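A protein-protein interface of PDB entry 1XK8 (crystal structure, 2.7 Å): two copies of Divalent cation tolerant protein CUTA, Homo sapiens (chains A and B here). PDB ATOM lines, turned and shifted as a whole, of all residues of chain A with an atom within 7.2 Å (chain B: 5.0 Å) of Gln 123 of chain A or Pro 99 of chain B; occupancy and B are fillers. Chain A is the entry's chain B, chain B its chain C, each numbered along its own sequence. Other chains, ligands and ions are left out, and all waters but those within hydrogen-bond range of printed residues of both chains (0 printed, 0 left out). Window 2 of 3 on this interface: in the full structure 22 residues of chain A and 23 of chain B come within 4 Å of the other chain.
Of the 11 printed residues of chain A, 6 touch a printed residue of chain B. Of the 13 printed residues of chain B, 7 touch a printed residue of chain A. Among the printed residues, no Asp or Glu carboxylate lies within 4 Å of a Lys or Arg side-chain nitrogen of the other chain.
The side-chain hydroxyl (OH) of Tyr 31 of chain A sits at hydrogen-bond distance from the backbone carbonyl oxygen (O) of Val 121 of chain A (2.9 Å). The backbone NH (N) of Ser 37 of chain B sits at hydrogen-bond distance from the side-chain hydroxyl (OG) of Ser 95 of chain B, at 3.3 Å. The backbone NH (N) of Gly 34 of chain A sits at hydrogen-bond distance from the backbone carbonyl oxygen (O) of Val 121 of chain A. O of Val 98 of chain B lies within hydrogen-bond range of OG1 of Thr 102 of chain B, 2.5 Å away.
Val 121 of chain A touches Ile 117 of chain B (CG1 to CB, 3.7 Å). Ala 118 of chain B touches Val 121 of chain A (O to CG1, 3.7 Å). OE1 of Gln 123 of chain A touches CB of Val 98 of chain B, at 3.4 Å. NE2 of Gln 123 of chain A touches CG of Pro 99 of chain B, at 3.8 Å. Ile 117 of chain B touches Gln 123 of chain A (C to O, 3.7 Å). Gly 124 of chain A touches Val 116 of chain B (CA to O, 3.1 Å). Asn 125 of chain A touches Thr 102 of chain B. CG2 of Ile 117 of chain B touches CD2 of Leu 129 of chain A, 3.8 Å away.
Printed residues of chain B within 4 Å of Gln 123 of chain A: Ser 95, Val 98, Pro 99, Ile 117 and Ala 118. Of chain A, only Gln 123 comes within 4 Å of Pro 99 of chain B. Of the printed residues of chain A, Ser 95 of chain B touches Gln 123 (2.9 Å). Of the printed residues of chain B, Val 121 of chain A touches Ile 117 (3.7 Å) and Ala 118 (3.7 Å). Of the printed residues of chain B, Glu 122 of chain A touches Ala 118. Phe 126 of chain A touches none of the printed residues of chain B. The nearest residue of chain A that does not touch Pro 99 of chain B is Gly 124 of chain A (6.5 Å). The nearest printed residue of chain A that does not touch Val 116 of chain B is Gln 123 of chain A (4.4 Å).
N of Glu 122 of chain A sits at hydrogen-bond distance from O of Ala 118 of chain B, 3.0 Å away. The backbone NH (N) of Asn 125 of chain A is in hydrogen-bond range of the backbone carbonyl oxygen (O) of Val 116 of chain B (2.9 Å). O of Gln 123 of chain A sits at hydrogen-bond distance from N of Ala 118 of chain B (2.8 Å). The backbone carbonyl oxygen (O) of Ser 95 of chain B lies close to the side-chain amide oxygen (OE1) of Gln 123 of chain A, at 2.9 Å.
No position is printed for both chains.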
ATOM      1  N   TYR A  31       7.154 -30.392  10.457  1.00  0.00           N
ATOM      2  CA  TYR A  31       6.523 -29.772  11.673  1.00  0.00           C
ATOM      3  C   TYR A  31       5.138 -30.320  11.941  1.00  0.00           C
ATOM      4  O   TYR A  31       4.278 -30.274  11.065  1.00  0.00           O
ATOM      5  CB  TYR A  31       6.410 -28.231  11.532  1.00  0.00           C
ATOM      6  CG  TYR A  31       5.714 -27.572  12.723  1.00  0.00           C
ATOM      7  CD1 TYR A  31       4.471 -26.933  12.576  1.00  0.00           C
ATOM      8  CD2 TYR A  31       6.285 -27.627  14.006  1.00  0.00           C
ATOM      9  CE1 TYR A  31       3.821 -26.347  13.684  1.00  0.00           C
ATOM     10  CE2 TYR A  31       5.649 -27.045  15.116  1.00  0.00           C
ATOM     11  CZ  TYR A  31       4.422 -26.409  14.950  1.00  0.00           C
ATOM     12  OH  TYR A  31       3.809 -25.848  16.042  1.00  0.00           O
ATOM     13  N   PRO A  33       1.651 -29.882  13.340  1.00  0.00           N
ATOM     14  CA  PRO A  33       0.774 -28.801  13.761  1.00  0.00           C
ATOM     15  C   PRO A  33       0.457 -28.812  15.255  1.00  0.00           C
ATOM     16  O   PRO A  33       0.131 -29.866  15.812  1.00  0.00           O
ATOM     17  CB  PRO A  33      -0.480 -29.035  12.930  1.00  0.00           C
ATOM     18  CG  PRO A  33       0.061 -29.640  11.655  1.00  0.00           C
ATOM     19  CD  PRO A  33       1.158 -30.539  12.113  1.00  0.00           C
ATOM     20  N   GLY A  34       0.587 -27.640  15.886  1.00  0.00           N
ATOM     21  CA  GLY A  34       0.197 -27.445  17.274  1.00  0.00           C
ATOM     22  C   GLY A  34       1.149 -28.000  18.307  1.00  0.00           C
ATOM     23  O   GLY A  34       0.818 -28.014  19.485  1.00  0.00           O
ATOM     24  N   PRO A 120      -2.128 -22.977  20.365  1.00  0.00           N
ATOM     25  CA  PRO A 120      -1.290 -23.836  19.532  1.00  0.00           C
ATOM     26  C   PRO A 120      -0.924 -23.183  18.194  1.00  0.00           C
ATOM     27  O   PRO A 120      -1.755 -22.500  17.577  1.00  0.00           O
ATOM     28  CB  PRO A 120      -2.164 -25.075  19.325  1.00  0.00           C
ATOM     29  CG  PRO A 120      -3.546 -24.546  19.312  1.00  0.00           C
ATOM     30  CD  PRO A 120      -3.552 -23.338  20.254  1.00  0.00           C
ATOM     31  N   VAL A 121       0.315 -23.395  17.763  1.00  0.00           N
ATOM     32  CA  VAL A 121       0.798 -22.852  16.499  1.00  0.00           C
ATOM     33  C   VAL A 121       0.562 -23.871  15.400  1.00  0.00           C
ATOM     34  O   VAL A 121       1.184 -24.935  15.395  1.00  0.00           O
ATOM     35  CB  VAL A 121       2.288 -22.515  16.549  1.00  0.00           C
ATOM     36  CG1 VAL A 121       2.719 -21.844  15.232  1.00  0.00           C
ATOM     37  CG2 VAL A 121       2.600 -21.617  17.747  1.00  0.00           C
ATOM     38  N   GLU A 122      -0.346 -23.546  14.481  1.00  0.00           N
ATOM     39  CA  GLU A 122      -0.766 -24.473  13.421  1.00  0.00           C
ATOM     40  C   GLU A 122       0.269 -24.484  12.276  1.00  0.00           C
ATOM     41  O   GLU A 122       0.591 -25.538  11.746  1.00  0.00           O
ATOM     42  CB  GLU A 122      -2.187 -24.095  12.906  1.00  0.00           C
ATOM     43  CG  GLU A 122      -3.014 -25.246  12.231  1.00  0.00           C
ATOM     44  CD  GLU A 122      -4.242 -24.725  11.407  1.00  0.00           C
ATOM     45  OE1 GLU A 122      -4.091 -23.660  10.756  1.00  0.00           O
ATOM     46  OE2 GLU A 122      -5.346 -25.378  11.408  1.00  0.00           O
ATOM     47  N   GLN A 123       0.771 -23.298  11.912  1.00  0.00           N
ATOM     48  CA  GLN A 123       1.769 -23.133  10.846  1.00  0.00           C
ATOM     49  C   GLN A 123       2.810 -22.096  11.248  1.00  0.00           C
ATOM     50  O   GLN A 123       2.592 -21.318  12.188  1.00  0.00           O
ATOM     51  CB  GLN A 123       1.129 -22.614   9.557  1.00  0.00           C
ATOM     52  CG  GLN A 123      -0.055 -23.357   9.041  1.00  0.00           C
ATOM     53  CD  GLN A 123      -0.406 -22.918   7.614  1.00  0.00           C
ATOM     54  OE1 GLN A 123      -1.372 -22.183   7.389  1.00  0.00           O
ATOM     55  NE2 GLN A 123       0.396 -23.355   6.651  1.00  0.00           N
ATOM     56  N   GLY A 124       3.923 -22.052  10.509  1.00  0.00           N
ATOM     57  CA  GLY A 124       4.965 -21.044  10.750  1.00  0.00           C
ATOM     58  C   GLY A 124       6.259 -21.241   9.987  1.00  0.00           C
ATOM     59  O   GLY A 124       6.321 -22.019   9.049  1.00  0.00           O
ATOM     60  N   ASN A 125       7.292 -20.508  10.394  1.00  0.00           N
ATOM     61  CA  ASN A 125       8.631 -20.644   9.822  1.00  0.00           C
ATOM     62  C   ASN A 125       9.308 -21.887  10.388  1.00  0.00           C
ATOM     63  O   ASN A 125       9.719 -21.902  11.553  1.00  0.00           O
ATOM     64  CB  ASN A 125       9.465 -19.391  10.133  1.00  0.00           C
ATOM     65  CG  ASN A 125      10.592 -19.169   9.137  1.00  0.00           C
ATOM     66  OD1 ASN A 125      10.804 -19.972   8.236  1.00  0.00           O
ATOM     67  ND2 ASN A 125      11.312 -18.060   9.292  1.00  0.00           N
ATOM     68  N   PHE A 126       9.421 -22.935   9.566  1.00  0.00           N
ATOM     69  CA  PHE A 126       9.895 -24.249  10.055  1.00  0.00           C
ATOM     70  C   PHE A 126      11.222 -24.186  10.820  1.00  0.00           C
ATOM     71  O   PHE A 126      11.323 -24.758  11.905  1.00  0.00           O
ATOM     72  CB  PHE A 126       9.984 -25.293   8.928  1.00  0.00           C
ATOM     73  CG  PHE A 126      10.608 -26.595   9.373  1.00  0.00           C
ATOM     74  CD1 PHE A 126      11.796 -27.070   8.790  1.00  0.00           C
ATOM     75  CD2 PHE A 126      10.032 -27.339  10.419  1.00  0.00           C
ATOM     76  CE1 PHE A 126      12.379 -28.270   9.226  1.00  0.00           C
ATOM     77  CE2 PHE A 126      10.616 -28.549  10.859  1.00  0.00           C
ATOM     78  CZ  PHE A 126      11.789 -29.006  10.267  1.00  0.00           C
ATOM     79  N   LEU A 129      10.471 -22.813  14.189  1.00  0.00           N
ATOM     80  CA  LEU A 129       9.716 -23.839  14.933  1.00  0.00           C
ATOM     81  C   LEU A 129      10.627 -24.998  15.362  1.00  0.00           C
ATOM     82  O   LEU A 129      10.505 -25.521  16.468  1.00  0.00           O
ATOM     83  CB  LEU A 129       8.545 -24.336  14.092  1.00  0.00           C
ATOM     84  CG  LEU A 129       7.529 -23.254  13.664  1.00  0.00           C
ATOM     85  CD1 LEU A 129       6.537 -23.802  12.653  1.00  0.00           C
ATOM     86  CD2 LEU A 129       6.799 -22.673  14.866  1.00  0.00           C
ATOM     87  N   SER B  37      -6.074 -16.920   9.818  1.00  0.00           N
ATOM     88  CA  SER B  37      -5.075 -17.041  10.879  1.00  0.00           C
ATOM     89  C   SER B  37      -4.580 -15.681  11.330  1.00  0.00           C
ATOM     90  O   SER B  37      -4.659 -14.701  10.597  1.00  0.00           O
ATOM     91  CB  SER B  37      -3.875 -17.887  10.421  1.00  0.00           C
ATOM     92  OG  SER B  37      -4.255 -19.219  10.123  1.00  0.00           O
ATOM     93  N   SER B  95      -5.463 -18.512   6.010  1.00  0.00           N
ATOM     94  CA  SER B  95      -4.548 -19.532   6.479  1.00  0.00           C
ATOM     95  C   SER B  95      -3.809 -20.160   5.292  1.00  0.00           C
ATOM     96  O   SER B  95      -2.648 -20.539   5.421  1.00  0.00           O
ATOM     97  CB  SER B  95      -5.294 -20.576   7.311  1.00  0.00           C
ATOM     98  OG  SER B  95      -5.824 -19.977   8.479  1.00  0.00           O
ATOM     99  N   SER B  96      -4.478 -20.232   4.135  1.00  0.00           N
ATOM    100  CA  SER B  96      -3.843 -20.708   2.889  1.00  0.00           C
ATOM    101  C   SER B  96      -2.662 -19.845   2.433  1.00  0.00           C
ATOM    102  O   SER B  96      -1.777 -20.333   1.747  1.00  0.00           O
ATOM    103  CB  SER B  96      -4.863 -20.777   1.755  1.00  0.00           C
ATOM    104  OG  SER B  96      -5.454 -19.512   1.546  1.00  0.00           O
ATOM    105  N   LEU B  97      -2.652 -18.570   2.816  1.00  0.00           N
ATOM    106  CA  LEU B  97      -1.558 -17.658   2.442  1.00  0.00           C
ATOM    107  C   LEU B  97      -0.374 -17.659   3.403  1.00  0.00           C
ATOM    108  O   LEU B  97       0.635 -17.029   3.128  1.00  0.00           O
ATOM    109  CB  LEU B  97      -2.073 -16.234   2.297  1.00  0.00           C
ATOM    110  CG  LEU B  97      -3.035 -16.054   1.134  1.00  0.00           C
ATOM    111  CD1 LEU B  97      -3.659 -14.677   1.176  1.00  0.00           C
ATOM    112  CD2 LEU B  97      -2.330 -16.300  -0.200  1.00  0.00           C
ATOM    113  N   VAL B  98      -0.485 -18.359   4.522  1.00  0.00           N
ATOM    114  CA  VAL B  98       0.563 -18.325   5.536  1.00  0.00           C
ATOM    115  C   VAL B  98       1.939 -18.773   5.004  1.00  0.00           C
ATOM    116  O   VAL B  98       2.947 -18.152   5.315  1.00  0.00           O
ATOM    117  CB  VAL B  98       0.159 -19.164   6.767  1.00  0.00           C
ATOM    118  CG1 VAL B  98       1.316 -19.290   7.753  1.00  0.00           C
ATOM    119  CG2 VAL B  98      -1.071 -18.546   7.445  1.00  0.00           C
ATOM    120  N   PRO B  99       1.988 -19.860   4.207  1.00  0.00           N
ATOM    121  CA  PRO B  99       3.278 -20.216   3.599  1.00  0.00           C
ATOM    122  C   PRO B  99       3.862 -19.090   2.712  1.00  0.00           C
ATOM    123  O   PRO B  99       5.062 -18.791   2.797  1.00  0.00           O
ATOM    124  CB  PRO B  99       2.941 -21.471   2.761  1.00  0.00           C
ATOM    125  CG  PRO B  99       1.708 -22.023   3.360  1.00  0.00           C
ATOM    126  CD  PRO B  99       0.931 -20.822   3.830  1.00  0.00           C
ATOM    127  N   ALA B 100       3.017 -18.479   1.883  1.00  0.00           N
ATOM    128  CA  ALA B 100       3.449 -17.378   1.020  1.00  0.00           C
ATOM    129  C   ALA B 100       3.875 -16.168   1.843  1.00  0.00           C
ATOM    130  O   ALA B 100       4.851 -15.491   1.503  1.00  0.00           O
ATOM    131  CB  ALA B 100       2.338 -16.995   0.037  1.00  0.00           C
ATOM    132  N   LEU B 101       3.137 -15.899   2.924  1.00  0.00           N
ATOM    133  CA  LEU B 101       3.466 -14.813   3.856  1.00  0.00           C
ATOM    134  C   LEU B 101       4.828 -15.045   4.484  1.00  0.00           C
ATOM    135  O   LEU B 101       5.658 -14.138   4.554  1.00  0.00           O
ATOM    136  CB  LEU B 101       2.399 -14.725   4.954  1.00  0.00           C
ATOM    137  CG  LEU B 101       2.593 -13.696   6.071  1.00  0.00           C
ATOM    138  CD1 LEU B 101       2.523 -12.298   5.523  1.00  0.00           C
ATOM    139  CD2 LEU B 101       1.544 -13.892   7.115  1.00  0.00           C
ATOM    140  N   THR B 102       5.048 -16.268   4.938  1.00  0.00           N
ATOM    141  CA  THR B 102       6.291 -16.631   5.599  1.00  0.00           C
ATOM    142  C   THR B 102       7.491 -16.517   4.643  1.00  0.00           C
ATOM    143  O   THR B 102       8.535 -15.982   5.030  1.00  0.00           O
ATOM    144  CB  THR B 102       6.187 -18.044   6.207  1.00  0.00           C
ATOM    145  OG1 THR B 102       4.928 -18.177   6.883  1.00  0.00           O
ATOM    146  CG2 THR B 102       7.310 -18.293   7.194  1.00  0.00           C
ATOM    147  N   ASP B 103       7.334 -16.996   3.401  1.00  0.00           N
ATOM    148  CA  ASP B 103       8.396 -16.868   2.375  1.00  0.00           C
ATOM    149  C   ASP B 103       8.781 -15.426   2.151  1.00  0.00           C
ATOM    150  O   ASP B 103       9.966 -15.084   2.121  1.00  0.00           O
ATOM    151  CB  ASP B 103       7.949 -17.463   1.045  1.00  0.00           C
ATOM    152  CG  ASP B 103       7.732 -18.947   1.127  1.00  0.00           C
ATOM    153  OD1 ASP B 103       8.323 -19.582   2.046  1.00  0.00           O
ATOM    154  OD2 ASP B 103       6.967 -19.472   0.277  1.00  0.00           O
ATOM    155  N   VAL B 116       7.997 -16.490  12.694  1.00  0.00           N
ATOM    156  CA  VAL B 116       6.664 -16.381  12.119  1.00  0.00           C
ATOM    157  C   VAL B 116       5.848 -17.551  12.635  1.00  0.00           C
ATOM    158  O   VAL B 116       6.147 -18.693  12.327  1.00  0.00           O
ATOM    159  CB  VAL B 116       6.678 -16.365  10.589  1.00  0.00           C
ATOM    160  CG1 VAL B 116       5.265 -16.142  10.043  1.00  0.00           C
ATOM    161  CG2 VAL B 116       7.613 -15.287  10.087  1.00  0.00           C
ATOM    162  N   ILE B 117       4.836 -17.253  13.446  1.00  0.00           N
ATOM    163  CA  ILE B 117       3.954 -18.277  13.993  1.00  0.00           C
ATOM    164  C   ILE B 117       2.501 -17.907  13.736  1.00  0.00           C
ATOM    165  O   ILE B 117       2.096 -16.791  13.969  1.00  0.00           O
ATOM    166  CB  ILE B 117       4.204 -18.504  15.496  1.00  0.00           C
ATOM    167  CG1 ILE B 117       4.115 -17.192  16.283  1.00  0.00           C
ATOM    168  CG2 ILE B 117       5.567 -19.141  15.698  1.00  0.00           C
ATOM    169  CD1 ILE B 117       4.107 -17.375  17.778  1.00  0.00           C
ATOM    170  N   ALA B 118       1.737 -18.860  13.219  1.00  0.00           N
ATOM    171  CA  ALA B 118       0.365 -18.614  12.797  1.00  0.00           C
ATOM    172  C   ALA B 118      -0.593 -19.347  13.708  1.00  0.00           C
ATOM    173  O   ALA B 118      -0.446 -20.550  13.945  1.00  0.00           O
ATOM    174  CB  ALA B 118       0.163 -19.052  11.338  1.00  0.00           C
